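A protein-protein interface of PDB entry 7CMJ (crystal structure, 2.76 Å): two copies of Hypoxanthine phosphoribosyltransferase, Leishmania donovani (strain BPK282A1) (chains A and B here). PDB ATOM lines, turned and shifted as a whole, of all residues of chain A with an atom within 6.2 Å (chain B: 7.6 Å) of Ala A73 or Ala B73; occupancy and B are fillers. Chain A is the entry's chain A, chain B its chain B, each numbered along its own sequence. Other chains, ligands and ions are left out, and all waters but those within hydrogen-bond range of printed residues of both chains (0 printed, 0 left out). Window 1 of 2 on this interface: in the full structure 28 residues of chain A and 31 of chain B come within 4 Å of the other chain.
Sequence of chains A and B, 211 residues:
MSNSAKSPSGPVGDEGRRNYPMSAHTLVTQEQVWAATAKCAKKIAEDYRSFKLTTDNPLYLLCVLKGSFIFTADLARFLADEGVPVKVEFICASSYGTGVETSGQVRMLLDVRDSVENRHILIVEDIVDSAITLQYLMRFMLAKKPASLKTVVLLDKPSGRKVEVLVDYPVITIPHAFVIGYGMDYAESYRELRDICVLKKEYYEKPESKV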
ATOM      1  N   SER A  68      -6.312 -20.525  28.784  1.00  0.00           N
ATOM      2  CA  SER A  68      -4.994 -21.099  28.522  1.00  0.00           C
ATOM      3  C   SER A  68      -3.943 -20.061  28.148  1.00  0.00           C
ATOM      4  O   SER A  68      -2.774 -20.427  27.962  1.00  0.00           O
ATOM      5  CB  SER A  68      -5.081 -22.147  27.416  1.00  0.00           C
ATOM      6  OG  SER A  68      -5.843 -23.255  27.859  1.00  0.00           O
ATOM      7  N   PHE A  69      -4.312 -18.781  28.056  1.00  0.00           N
ATOM      8  CA  PHE A  69      -3.450 -17.874  27.312  1.00  0.00           C
ATOM      9  C   PHE A  69      -2.186 -17.507  28.085  1.00  0.00           C
ATOM     10  O   PHE A  69      -1.087 -17.517  27.522  1.00  0.00           O
ATOM     11  CB  PHE A  69      -4.249 -16.655  26.859  1.00  0.00           C
ATOM     12  CG  PHE A  69      -4.244 -15.490  27.806  1.00  0.00           C
ATOM     13  CD1 PHE A  69      -3.403 -14.408  27.586  1.00  0.00           C
ATOM     14  CD2 PHE A  69      -5.134 -15.435  28.859  1.00  0.00           C
ATOM     15  CE1 PHE A  69      -3.423 -13.317  28.427  1.00  0.00           C
ATOM     16  CE2 PHE A  69      -5.167 -14.350  29.694  1.00  0.00           C
ATOM     17  CZ  PHE A  69      -4.310 -13.287  29.485  1.00  0.00           C
ATOM     18  N   ILE A  70      -2.295 -17.222  29.376  1.00  0.00           N
ATOM     19  CA  ILE A  70      -1.067 -17.005  30.118  1.00  0.00           C
ATOM     20  C   ILE A  70      -0.241 -18.278  30.135  1.00  0.00           C
ATOM     21  O   ILE A  70       0.975 -18.252  29.900  1.00  0.00           O
ATOM     22  CB  ILE A  70      -1.390 -16.489  31.524  1.00  0.00           C
ATOM     23  CG1 ILE A  70      -1.747 -15.006  31.426  1.00  0.00           C
ATOM     24  CG2 ILE A  70      -0.224 -16.772  32.478  1.00  0.00           C
ATOM     25  CD1 ILE A  70      -2.232 -14.424  32.717  1.00  0.00           C
ATOM     26  N   PHE A  71      -0.895 -19.419  30.360  1.00  0.00           N
ATOM     27  CA  PHE A  71      -0.174 -20.687  30.396  1.00  0.00           C
ATOM     28  C   PHE A  71       0.491 -20.976  29.064  1.00  0.00           C
ATOM     29  O   PHE A  71       1.613 -21.497  29.029  1.00  0.00           O
ATOM     30  CB  PHE A  71      -1.122 -21.821  30.766  1.00  0.00           C
ATOM     31  CG  PHE A  71      -0.491 -23.179  30.749  1.00  0.00           C
ATOM     32  CD1 PHE A  71       0.775 -23.383  31.259  1.00  0.00           C
ATOM     33  CD2 PHE A  71      -1.188 -24.273  30.247  1.00  0.00           C
ATOM     34  CE1 PHE A  71       1.350 -24.654  31.253  1.00  0.00           C
ATOM     35  CE2 PHE A  71      -0.625 -25.538  30.241  1.00  0.00           C
ATOM     36  CZ  PHE A  71       0.646 -25.728  30.745  1.00  0.00           C
ATOM     37  N   THR A  72      -0.189 -20.645  27.957  1.00  0.00           N
ATOM     38  CA  THR A  72       0.396 -20.836  26.633  1.00  0.00           C
ATOM     39  C   THR A  72       1.629 -19.962  26.470  1.00  0.00           C
ATOM     40  O   THR A  72       2.690 -20.437  26.035  1.00  0.00           O
ATOM     41  CB  THR A  72      -0.637 -20.531  25.532  1.00  0.00           C
ATOM     42  OG1 THR A  72      -1.641 -21.550  25.520  1.00  0.00           O
ATOM     43  CG2 THR A  72       0.016 -20.489  24.163  1.00  0.00           C
ATOM     44  N   ALA A  73       1.516 -18.684  26.853  1.00  0.00           N
ATOM     45  CA  ALA A  73       2.635 -17.762  26.678  1.00  0.00           C
ATOM     46  C   ALA A  73       3.862 -18.224  27.461  1.00  0.00           C
ATOM     47  O   ALA A  73       4.990 -18.181  26.947  1.00  0.00           O
ATOM     48  CB  ALA A  73       2.228 -16.346  27.080  1.00  0.00           C
ATOM     49  N   ASP A  74       3.670 -18.709  28.689  1.00  0.00           N
ATOM     50  CA  ASP A  74       4.836 -19.205  29.413  1.00  0.00           C
ATOM     51  C   ASP A  74       5.300 -20.553  28.873  1.00  0.00           C
ATOM     52  O   ASP A  74       6.508 -20.763  28.712  1.00  0.00           O
ATOM     53  CB  ASP A  74       4.557 -19.308  30.909  1.00  0.00           C
ATOM     54  CG  ASP A  74       4.251 -17.967  31.542  1.00  0.00           C
ATOM     55  OD1 ASP A  74       3.938 -17.965  32.741  1.00  0.00           O
ATOM     56  OD2 ASP A  74       4.290 -16.920  30.856  1.00  0.00           O
ATOM     57  N   LEU A  75       4.376 -21.480  28.579  1.00  0.00           N
ATOM     58  CA  LEU A  75       4.812 -22.808  28.137  1.00  0.00           C
ATOM     59  C   LEU A  75       5.578 -22.723  26.824  1.00  0.00           C
ATOM     60  O   LEU A  75       6.591 -23.411  26.641  1.00  0.00           O
ATOM     61  CB  LEU A  75       3.628 -23.770  28.007  1.00  0.00           C
ATOM     62  CG  LEU A  75       3.836 -25.088  27.231  1.00  0.00           C
ATOM     63  CD1 LEU A  75       4.948 -25.920  27.820  1.00  0.00           C
ATOM     64  CD2 LEU A  75       2.580 -25.940  27.179  1.00  0.00           C
ATOM     65  N   ALA A  76       5.136 -21.856  25.913  1.00  0.00           N
ATOM     66  CA  ALA A  76       5.871 -21.686  24.665  1.00  0.00           C
ATOM     67  C   ALA A  76       7.320 -21.264  24.926  1.00  0.00           C
ATOM     68  O   ALA A  76       8.244 -21.769  24.278  1.00  0.00           O
ATOM     69  CB  ALA A  76       5.141 -20.678  23.774  1.00  0.00           C
ATOM     70  N   ARG A  77       7.542 -20.373  25.902  1.00  0.00           N
ATOM     71  CA  ARG A  77       8.907 -19.925  26.194  1.00  0.00           C
ATOM     72  C   ARG A  77       9.722 -21.004  26.910  1.00  0.00           C
ATOM     73  O   ARG A  77      10.953 -21.052  26.768  1.00  0.00           O
ATOM     74  CB  ARG A  77       8.876 -18.621  27.002  1.00  0.00           C
ATOM     75  CG  ARG A  77       8.272 -17.460  26.201  1.00  0.00           C
ATOM     76  CD  ARG A  77       8.099 -16.195  27.022  1.00  0.00           C
ATOM     77  NE  ARG A  77       6.819 -16.152  27.732  1.00  0.00           N
ATOM     78  CZ  ARG A  77       6.394 -15.116  28.455  1.00  0.00           C
ATOM     79  NH1 ARG A  77       7.144 -14.022  28.577  1.00  0.00           N
ATOM     80  NH2 ARG A  77       5.224 -15.176  29.072  1.00  0.00           N
ATOM     81  N   PHE A  78       9.068 -21.888  27.660  1.00  0.00           N
ATOM     82  CA  PHE A  78       9.808 -23.017  28.210  1.00  0.00           C
ATOM     83  C   PHE A  78      10.161 -24.010  27.111  1.00  0.00           C
ATOM     84  O   PHE A  78      11.241 -24.622  27.140  1.00  0.00           O
ATOM     85  CB  PHE A  78       9.004 -23.689  29.327  1.00  0.00           C
ATOM     86  CG  PHE A  78       8.935 -22.877  30.590  1.00  0.00           C
ATOM     87  CD1 PHE A  78      10.093 -22.541  31.277  1.00  0.00           C
ATOM     88  CD2 PHE A  78       7.716 -22.424  31.076  1.00  0.00           C
ATOM     89  CE1 PHE A  78      10.036 -21.790  32.430  1.00  0.00           C
ATOM     90  CE2 PHE A  78       7.658 -21.662  32.236  1.00  0.00           C
ATOM     91  CZ  PHE A  78       8.816 -21.349  32.910  1.00  0.00           C
ATOM     92  N   GLU A 192      -5.402 -11.989  35.817  1.00  0.00           N
ATOM     93  CA  GLU A 192      -4.102 -11.332  35.798  1.00  0.00           C
ATOM     94  C   GLU A 192      -3.222 -11.700  36.987  1.00  0.00           C
ATOM     95  O   GLU A 192      -2.053 -11.301  37.012  1.00  0.00           O
ATOM     96  CB  GLU A 192      -4.287  -9.812  35.742  1.00  0.00           C
ATOM     97  CG  GLU A 192      -4.768  -9.167  37.045  1.00  0.00           C
ATOM     98  CD  GLU A 192      -6.279  -9.211  37.241  1.00  0.00           C
ATOM     99  OE1 GLU A 192      -6.944 -10.016  36.571  1.00  0.00           O
ATOM    100  OE2 GLU A 192      -6.800  -8.443  38.082  1.00  0.00           O
ATOM    101  N   LEU B  61      -8.131  -5.254  28.934  1.00  0.00           N
ATOM    102  CA  LEU B  61      -7.017  -5.415  28.009  1.00  0.00           C
ATOM    103  C   LEU B  61      -7.529  -6.099  26.753  1.00  0.00           C
ATOM    104  O   LEU B  61      -7.979  -7.248  26.808  1.00  0.00           O
ATOM    105  CB  LEU B  61      -5.896  -6.239  28.636  1.00  0.00           C
ATOM    106  CG  LEU B  61      -5.050  -5.584  29.730  1.00  0.00           C
ATOM    107  CD1 LEU B  61      -3.762  -6.377  29.878  1.00  0.00           C
ATOM    108  CD2 LEU B  61      -4.760  -4.107  29.426  1.00  0.00           C
ATOM    109  N   CYS B  63      -6.594  -7.769  23.601  1.00  0.00           N
ATOM    110  CA  CYS B  63      -5.426  -8.408  23.007  1.00  0.00           C
ATOM    111  C   CYS B  63      -5.691  -8.728  21.541  1.00  0.00           C
ATOM    112  O   CYS B  63      -6.573  -9.532  21.235  1.00  0.00           O
ATOM    113  CB  CYS B  63      -5.079  -9.678  23.784  1.00  0.00           C
ATOM    114  SG  CYS B  63      -3.871 -10.726  22.973  1.00  0.00           S
ATOM    115  N   SER B  68       0.139 -10.196  19.881  1.00  0.00           N
ATOM    116  CA  SER B  68       0.131  -9.544  21.185  1.00  0.00           C
ATOM    117  C   SER B  68      -0.014 -10.509  22.363  1.00  0.00           C
ATOM    118  O   SER B  68       0.011 -10.052  23.511  1.00  0.00           O
ATOM    119  CB  SER B  68      -1.003  -8.522  21.254  1.00  0.00           C
ATOM    120  OG  SER B  68      -0.715  -7.399  20.454  1.00  0.00           O
ATOM    121  N   PHE B  69      -0.172 -11.817  22.139  1.00  0.00           N
ATOM    122  CA  PHE B  69      -0.638 -12.640  23.248  1.00  0.00           C
ATOM    123  C   PHE B  69       0.411 -12.773  24.353  1.00  0.00           C
ATOM    124  O   PHE B  69       0.070 -12.755  25.543  1.00  0.00           O
ATOM    125  CB  PHE B  69      -1.124 -13.998  22.734  1.00  0.00           C
ATOM    126  CG  PHE B  69      -0.063 -15.059  22.615  1.00  0.00           C
ATOM    127  CD1 PHE B  69       0.049 -16.050  23.581  1.00  0.00           C
ATOM    128  CD2 PHE B  69       0.755 -15.122  21.494  1.00  0.00           C
ATOM    129  CE1 PHE B  69       0.987 -17.059  23.459  1.00  0.00           C
ATOM    130  CE2 PHE B  69       1.694 -16.131  21.360  1.00  0.00           C
ATOM    131  CZ  PHE B  69       1.816 -17.100  22.348  1.00  0.00           C
ATOM    132  N   ILE B  70       1.686 -12.862  24.000  1.00  0.00           N
ATOM    133  CA  ILE B  70       2.688 -12.952  25.049  1.00  0.00           C
ATOM    134  C   ILE B  70       2.843 -11.614  25.766  1.00  0.00           C
ATOM    135  O   ILE B  70       2.989 -11.569  26.998  1.00  0.00           O
ATOM    136  CB  ILE B  70       4.009 -13.468  24.463  1.00  0.00           C
ATOM    137  CG1 ILE B  70       3.820 -14.934  24.075  1.00  0.00           C
ATOM    138  CG2 ILE B  70       5.180 -13.245  25.445  1.00  0.00           C
ATOM    139  CD1 ILE B  70       4.965 -15.520  23.317  1.00  0.00           C
ATOM    140  N   PHE B  71       2.792 -10.501  25.019  1.00  0.00           N
ATOM    141  CA  PHE B  71       2.844  -9.184  25.659  1.00  0.00           C
ATOM    142  C   PHE B  71       1.701  -9.027  26.648  1.00  0.00           C
ATOM    143  O   PHE B  71       1.909  -8.632  27.802  1.00  0.00           O
ATOM    144  CB  PHE B  71       2.800  -8.075  24.603  1.00  0.00           C
ATOM    145  CG  PHE B  71       2.995  -6.682  25.151  1.00  0.00           C
ATOM    146  CD1 PHE B  71       3.708  -6.462  26.312  1.00  0.00           C
ATOM    147  CD2 PHE B  71       2.465  -5.581  24.488  1.00  0.00           C
ATOM    148  CE1 PHE B  71       3.887  -5.168  26.809  1.00  0.00           C
ATOM    149  CE2 PHE B  71       2.639  -4.289  24.979  1.00  0.00           C
ATOM    150  CZ  PHE B  71       3.355  -4.091  26.141  1.00  0.00           C
ATOM    151  N   THR B  72       0.483  -9.350  26.200  1.00  0.00           N
ATOM    152  CA  THR B  72      -0.711  -9.241  27.031  1.00  0.00           C
ATOM    153  C   THR B  72      -0.553 -10.056  28.307  1.00  0.00           C
ATOM    154  O   THR B  72      -0.813  -9.560  29.413  1.00  0.00           O
ATOM    155  CB  THR B  72      -1.943  -9.705  26.228  1.00  0.00           C
ATOM    156  OG1 THR B  72      -2.138  -8.861  25.084  1.00  0.00           O
ATOM    157  CG2 THR B  72      -3.205  -9.683  27.076  1.00  0.00           C
ATOM    158  N   ALA B  73      -0.100 -11.306  28.170  1.00  0.00           N
ATOM    159  CA  ALA B  73       0.080 -12.166  29.335  1.00  0.00           C
ATOM    160  C   ALA B  73       1.063 -11.556  30.336  1.00  0.00           C
ATOM    161  O   ALA B  73       0.827 -11.587  31.553  1.00  0.00           O
ATOM    162  CB  ALA B  73       0.554 -13.553  28.892  1.00  0.00           C
ATOM    163  N   ASP B  74       2.173 -11.000  29.850  1.00  0.00           N
ATOM    164  CA  ASP B  74       3.120 -10.422  30.783  1.00  0.00           C
ATOM    165  C   ASP B  74       2.613  -9.085  31.309  1.00  0.00           C
ATOM    166  O   ASP B  74       2.764  -8.787  32.507  1.00  0.00           O
ATOM    167  CB  ASP B  74       4.494 -10.278  30.121  1.00  0.00           C
ATOM    168  CG  ASP B  74       5.187 -11.626  29.878  1.00  0.00           C
ATOM    169  OD1 ASP B  74       4.635 -12.688  30.265  1.00  0.00           O
ATOM    170  OD2 ASP B  74       6.294 -11.619  29.298  1.00  0.00           O
ATOM    171  N   LEU B  75       1.999  -8.270  30.439  1.00  0.00           N
ATOM    172  CA  LEU B  75       1.554  -6.954  30.884  1.00  0.00           C
ATOM    173  C   LEU B  75       0.461  -7.074  31.937  1.00  0.00           C
ATOM    174  O   LEU B  75       0.473  -6.341  32.936  1.00  0.00           O
ATOM    175  CB  LEU B  75       1.078  -6.122  29.695  1.00  0.00           C
ATOM    176  CG  LEU B  75       0.335  -4.791  29.952  1.00  0.00           C
ATOM    177  CD1 LEU B  75       1.150  -3.742  30.719  1.00  0.00           C
ATOM    178  CD2 LEU B  75      -0.128  -4.205  28.632  1.00  0.00           C
ATOM    179  N   ALA B  76      -0.484  -8.001  31.733  1.00  0.00           N
ATOM    180  CA  ALA B  76      -1.523  -8.262  32.724  1.00  0.00           C
ATOM    181  C   ALA B  76      -0.932  -8.476  34.107  1.00  0.00           C
ATOM    182  O   ALA B  76      -1.364  -7.857  35.091  1.00  0.00           O
ATOM    183  CB  ALA B  76      -2.330  -9.493  32.324  1.00  0.00           C
ATOM    184  N   ARG B  77       0.061  -9.367  34.198  1.00  0.00           N
ATOM    185  CA  ARG B  77       0.633  -9.702  35.497  1.00  0.00           C
ATOM    186  C   ARG B  77       1.414  -8.531  36.083  1.00  0.00           C
ATOM    187  O   ARG B  77       1.423  -8.350  37.307  1.00  0.00           O
ATOM    188  CB  ARG B  77       1.506 -10.956  35.380  1.00  0.00           C
ATOM    189  CG  ARG B  77       0.698 -12.238  35.165  1.00  0.00           C
ATOM    190  CD  ARG B  77       1.584 -13.447  34.858  1.00  0.00           C
ATOM    191  NE  ARG B  77       2.124 -13.447  33.494  1.00  0.00           N
ATOM    192  CZ  ARG B  77       2.750 -14.490  32.945  1.00  0.00           C
ATOM    193  NH1 ARG B  77       2.909 -15.612  33.652  1.00  0.00           N
ATOM    194  NH2 ARG B  77       3.227 -14.408  31.699  1.00  0.00           N
ATOM    195  N   PHE B  78       2.053  -7.716  35.233  1.00  0.00           N
ATOM    196  CA  PHE B  78       2.640  -6.468  35.716  1.00  0.00           C
ATOM    197  C   PHE B  78       1.563  -5.513  36.215  1.00  0.00           C
ATOM    198  O   PHE B  78       1.753  -4.819  37.222  1.00  0.00           O
ATOM    199  CB  PHE B  78       3.469  -5.803  34.614  1.00  0.00           C
ATOM    200  CG  PHE B  78       4.821  -6.434  34.399  1.00  0.00           C
ATOM    201  CD1 PHE B  78       5.746  -6.504  35.436  1.00  0.00           C
ATOM    202  CD2 PHE B  78       5.166  -6.960  33.160  1.00  0.00           C
ATOM    203  CE1 PHE B  78       6.979  -7.082  35.244  1.00  0.00           C
ATOM    204  CE2 PHE B  78       6.408  -7.540  32.965  1.00  0.00           C
ATOM    205  CZ  PHE B  78       7.318  -7.597  34.011  1.00  0.00           C
ATOM    206  N   LEU B  79       0.416  -5.470  35.526  1.00  0.00           N
ATOM    207  CA  LEU B  79      -0.701  -4.668  36.010  1.00  0.00           C
ATOM    208  C   LEU B  79      -1.253  -5.211  37.322  1.00  0.00           C
ATOM    209  O   LEU B  79      -1.706  -4.434  38.174  1.00  0.00           O
ATOM    210  CB  LEU B  79      -1.785  -4.602  34.945  1.00  0.00           C
ATOM    211  CG  LEU B  79      -1.432  -3.485  33.969  1.00  0.00           C
ATOM    212  CD1 LEU B  79      -2.269  -3.532  32.692  1.00  0.00           C
ATOM    213  CD2 LEU B  79      -1.570  -2.158  34.700  1.00  0.00           C
ATOM    214  N   VAL B  88      -9.641  -9.392  30.458  1.00  0.00           N
ATOM    215  CA  VAL B  88      -8.854  -9.665  29.261  1.00  0.00           C
ATOM    216  C   VAL B  88      -9.797 -10.083  28.142  1.00  0.00           C
ATOM    217  O   VAL B  88     -10.478 -11.114  28.258  1.00  0.00           O
ATOM    218  CB  VAL B  88      -7.807 -10.763  29.520  1.00  0.00           C
ATOM    219  CG1 VAL B  88      -6.977 -11.007  28.277  1.00  0.00           C
ATOM    220  CG2 VAL B  88      -6.933 -10.406  30.686  1.00  0.00           C
ATOM    221  N   PHE B  90     -10.101 -10.763  23.771  1.00  0.00           N
ATOM    222  CA  PHE B  90      -9.328 -11.088  22.578  1.00  0.00           C
ATOM    223  C   PHE B  90     -10.125 -10.742  21.332  1.00  0.00           C
ATOM    224  O   PHE B  90     -11.346 -10.956  21.279  1.00  0.00           O
ATOM    225  CB  PHE B  90      -8.938 -12.564  22.553  1.00  0.00           C
ATOM    226  CG  PHE B  90      -8.151 -12.988  23.751  1.00  0.00           C
ATOM    227  CD1 PHE B  90      -6.761 -12.963  23.730  1.00  0.00           C
ATOM    228  CD2 PHE B  90      -8.802 -13.388  24.913  1.00  0.00           C
ATOM    229  CE1 PHE B  90      -6.036 -13.333  24.829  1.00  0.00           C
ATOM    230  CE2 PHE B  90      -8.090 -13.765  26.014  1.00  0.00           C
ATOM    231  CZ  PHE B  90      -6.692 -13.738  25.975  1.00  0.00           C
ATOM    232  N   VAL B 124      -4.076  -3.582  23.095  1.00  0.00           N
ATOM    233  CA  VAL B 124      -2.730  -4.100  23.310  1.00  0.00           C
ATOM    234  C   VAL B 124      -2.159  -4.528  21.967  1.00  0.00           C
ATOM    235  O   VAL B 124      -2.530  -5.576  21.432  1.00  0.00           O
ATOM    236  CB  VAL B 124      -2.730  -5.284  24.288  1.00  0.00           C
ATOM    237  CG1 VAL B 124      -1.312  -5.828  24.458  1.00  0.00           C
ATOM    238  CG2 VAL B 124      -3.360  -4.899  25.617  1.00  0.00           C
ATOM    239  N   TYR B 182       8.950 -13.165  21.125  1.00  0.00           N
ATOM    240  CA  TYR B 182       8.069 -12.578  22.130  1.00  0.00           C
ATOM    241  C   TYR B 182       6.658 -12.407  21.564  1.00  0.00           C
ATOM    242  O   TYR B 182       6.049 -11.343  21.636  1.00  0.00           O
ATOM    243  CB  TYR B 182       8.643 -11.250  22.648  1.00  0.00           C
ATOM    244  CG  TYR B 182       8.048 -10.807  23.959  1.00  0.00           C
ATOM    245  CD1 TYR B 182       8.480 -11.351  25.159  1.00  0.00           C
ATOM    246  CD2 TYR B 182       7.033  -9.848  23.994  1.00  0.00           C
ATOM    247  CE1 TYR B 182       7.926 -10.948  26.368  1.00  0.00           C
ATOM    248  CE2 TYR B 182       6.473  -9.443  25.187  1.00  0.00           C
ATOM    249  CZ  TYR B 182       6.924 -10.001  26.375  1.00  0.00           C
ATOM    250  OH  TYR B 182       6.369  -9.612  27.567  1.00  0.00           O
ATOM    251  N   ARG B 191       7.335 -17.140  17.319  1.00  0.00           N
ATOM    252  CA  ARG B 191       6.611 -16.429  18.369  1.00  0.00           C
ATOM    253  C   ARG B 191       7.100 -16.816  19.754  1.00  0.00           C
ATOM    254  O   ARG B 191       6.941 -16.032  20.701  1.00  0.00           O
ATOM    255  CB  ARG B 191       5.106 -16.702  18.264  1.00  0.00           C
ATOM    256  CG  ARG B 191       4.465 -16.320  16.928  1.00  0.00           C
ATOM    257  CD  ARG B 191       2.957 -16.403  17.021  1.00  0.00           C
ATOM    258  NE  ARG B 191       2.319 -16.223  15.718  1.00  0.00           N
ATOM    259  CZ  ARG B 191       2.139 -15.044  15.134  1.00  0.00           C
ATOM    260  NH1 ARG B 191       2.546 -13.929  15.736  1.00  0.00           N
ATOM    261  NH2 ARG B 191       1.561 -14.979  13.949  1.00  0.00           N
ATOM    262  N   GLU B 192       7.732 -17.984  19.882  1.00  0.00           N
ATOM    263  CA  GLU B 192       8.011 -18.608  21.168  1.00  0.00           C
ATOM    264  C   GLU B 192       9.305 -18.126  21.820  1.00  0.00           C
ATOM    265  O   GLU B 192       9.565 -18.504  22.970  1.00  0.00           O
ATOM    266  CB  GLU B 192       8.041 -20.140  21.001  1.00  0.00           C
ATOM    267  CG  GLU B 192       9.266 -20.700  20.260  1.00  0.00           C
ATOM    268  CD  GLU B 192       9.126 -20.718  18.735  1.00  0.00           C
ATOM    269  OE1 GLU B 192       9.809 -21.528  18.069  1.00  0.00           O
ATOM    270  OE2 GLU B 192       8.347 -19.916  18.193  1.00  0.00           O
ATOM    271  N   LEU B 193      10.096 -17.291  21.137  1.00  0.00           N
ATOM    272  CA  LEU B 193      11.397 -16.867  21.659  1.00  0.00           C
ATOM    273  C   LEU B 193      11.255 -15.852  22.793  1.00  0.00           C
ATOM    274  O   LEU B 193      10.396 -14.969  22.749  1.00  0.00           O
ATOM    275  CB  LEU B 193      12.246 -16.274  20.540  1.00  0.00           C
ATOM    276  CG  LEU B 193      12.417 -17.097  19.259  1.00  0.00           C
ATOM    277  CD1 LEU B 193      13.435 -16.432  18.352  1.00  0.00           C
ATOM    278  CD2 LEU B 193      12.824 -18.537  19.545  1.00  0.00           C
ATOM    279  N   ARG B 194      12.127 -15.967  23.804  1.00  0.00           N
ATOM    280  CA  ARG B 194      12.029 -15.111  24.987  1.00  0.00           C
ATOM    281  C   ARG B 194      12.497 -13.690  24.699  1.00  0.00           C
ATOM    282  O   ARG B 194      11.961 -12.730  25.265  1.00  0.00           O
ATOM    283  CB  ARG B 194      12.848 -15.698  26.152  1.00  0.00           C
ATOM    284  CG  ARG B 194      12.263 -16.934  26.790  1.00  0.00           C
ATOM    285  CD  ARG B 194      13.234 -17.511  27.775  1.00  0.00           C
ATOM    286  NE  ARG B 194      12.679 -18.614  28.558  1.00  0.00           N
ATOM    287  CZ  ARG B 194      11.705 -18.487  29.454  1.00  0.00           C
ATOM    288  NH1 ARG B 194      11.145 -17.302  29.678  1.00  0.00           N
ATOM    289  NH2 ARG B 194      11.282 -19.554  30.116  1.00  0.00           N
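NH2 of Arg A77 sits close to NH2 of Arg B77 (3.4 Å). The guanidinium group of Arg B194 sits at hydrogen-bond distance from the backbone carbonyl oxygen of Arg A77 (3.5 Å). The side-chain carboxylate of Asp A74 lies within salt-bridge range of the guanidinium group of Arg B77 (2.7 Å). OD2 of Asp B74 lies within salt-bridge range of NH1 of Arg A77, at 2.6 Å.
The side-chain hydroxyl (OG1) of Thr B72 is in hydrogen-bond range of the backbone carbonyl oxygen (O) of Ser B68, at 2.9 Å. The backbone NH of Tyr B182 sits at hydrogen-bond distance from the backbone carbonyl oxygen of Leu B193 (2.8 Å). The side-chain carboxylate of Asp A74 is in salt-bridge range of the guanidinium group of Arg A77 (2.7 Å). OD2 of Asp B74 sits at hydrogen-bond distance from OH of Tyr B182, at 2.7 Å. The backbone carbonyl oxygen (O) of Ala A73 sits at hydrogen-bond distance from the guanidinium group (NE) of Arg A77 (2.8 Å). The side-chain hydroxyl (OG1) of Thr A72 lies within hydrogen-bond range of the backbone carbonyl oxygen (O) of Ser A68 (2.9 Å).
Among the printed residues, merely in contact across the chains: Phe A69 with Thr B72, Phe A69 with Ala B73, Phe A69 with Val B88, Phe A69 with Phe B90, Ile A70 with Ala B73, Ile A70 with Arg B77, Thr A72 with Phe B69, Ala A73 with Phe B69, Ala A73 with Ile B70, Ala A73 with Ala B73, Ala A76 with Glu B192, Arg A77 with Ile B70, Arg A77 with Tyr B182, Arg A77 with Glu B192, Phe A78 with Arg B194, Glu A192 with Ala B76 and Glu A192 with Arg B77.
Of the printed residues of chain B, Phe A69 touches Thr B72, Ala B73, Val B88 and Phe B90. Phe A71 touches none of the printed residues of chain B. Of the printed residues of chain B, Ala A76 touches Glu B192 (3.7 Å). Printed residues of chain A within 4 Å of Thr B72: Phe A69 (3.9 Å). Ala B73 touches just these residues of chain A: Phe A69, Ile A70 and Ala A73. Of the printed residues of chain A, Ala B76 touches Glu A192 (3.6 Å). Of the printed residues of chain A, Arg B194 touches Arg A77 (3.5 Å) and Phe A78 (3.4 Å). The nearest residue of chain B that does not touch Ala A73 is Arg B77 (5.1 Å). The nearest residue of chain A that does not touch Ala B73 is Arg A77 (4.9 Å). The nearest printed residue of chain A that does not touch Asp B74 is Asp A74 (4.3 Å).
Of the 22 printed residues of chain B, 12 touch a printed residue of chain A. Printed residues of chain B that touch a printed residue of chain A: Phe B69, Ile B70, Thr B72, Ala B73, Asp B74, Ala B76, Arg B77, Val B88, Phe B90, Tyr B182, Glu B192 and Arg B194. Hydrophobic or aromatic side chains of chain B that line the printed part of chain A: Phe B69, Ile B70, Ala B73, Ala B76, Val B88, Phe B90 and Tyr B182. Among the printed residues, Asp or Glu carboxylates within 4 Å of a Lys or Arg side-chain nitrogen of the other chain: Asp A74 with Arg B77 (2.7 Å) and Arg A77 with Asp B74 (2.6 Å).
Phe A69 touches Ala B73, and with the chains exchanged Ala A73 touches Phe B69. Ile A70 touches Ala B73, and with the chains exchanged Ala A73 touches Ile B70. Ala B73 touches its own counterpart, Ala A73. Arg A77 touches Glu B192, and with the chains exchanged Glu A192 touches Arg B77. Positions printed for both chains: 68, 69, 70, 71, 72, 73, 74, 75, 76, 77, 78 and 192. Of the 21 pairs that touch across the chains among the printed residues, 16 have their exchanged pair printed and touching as well.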
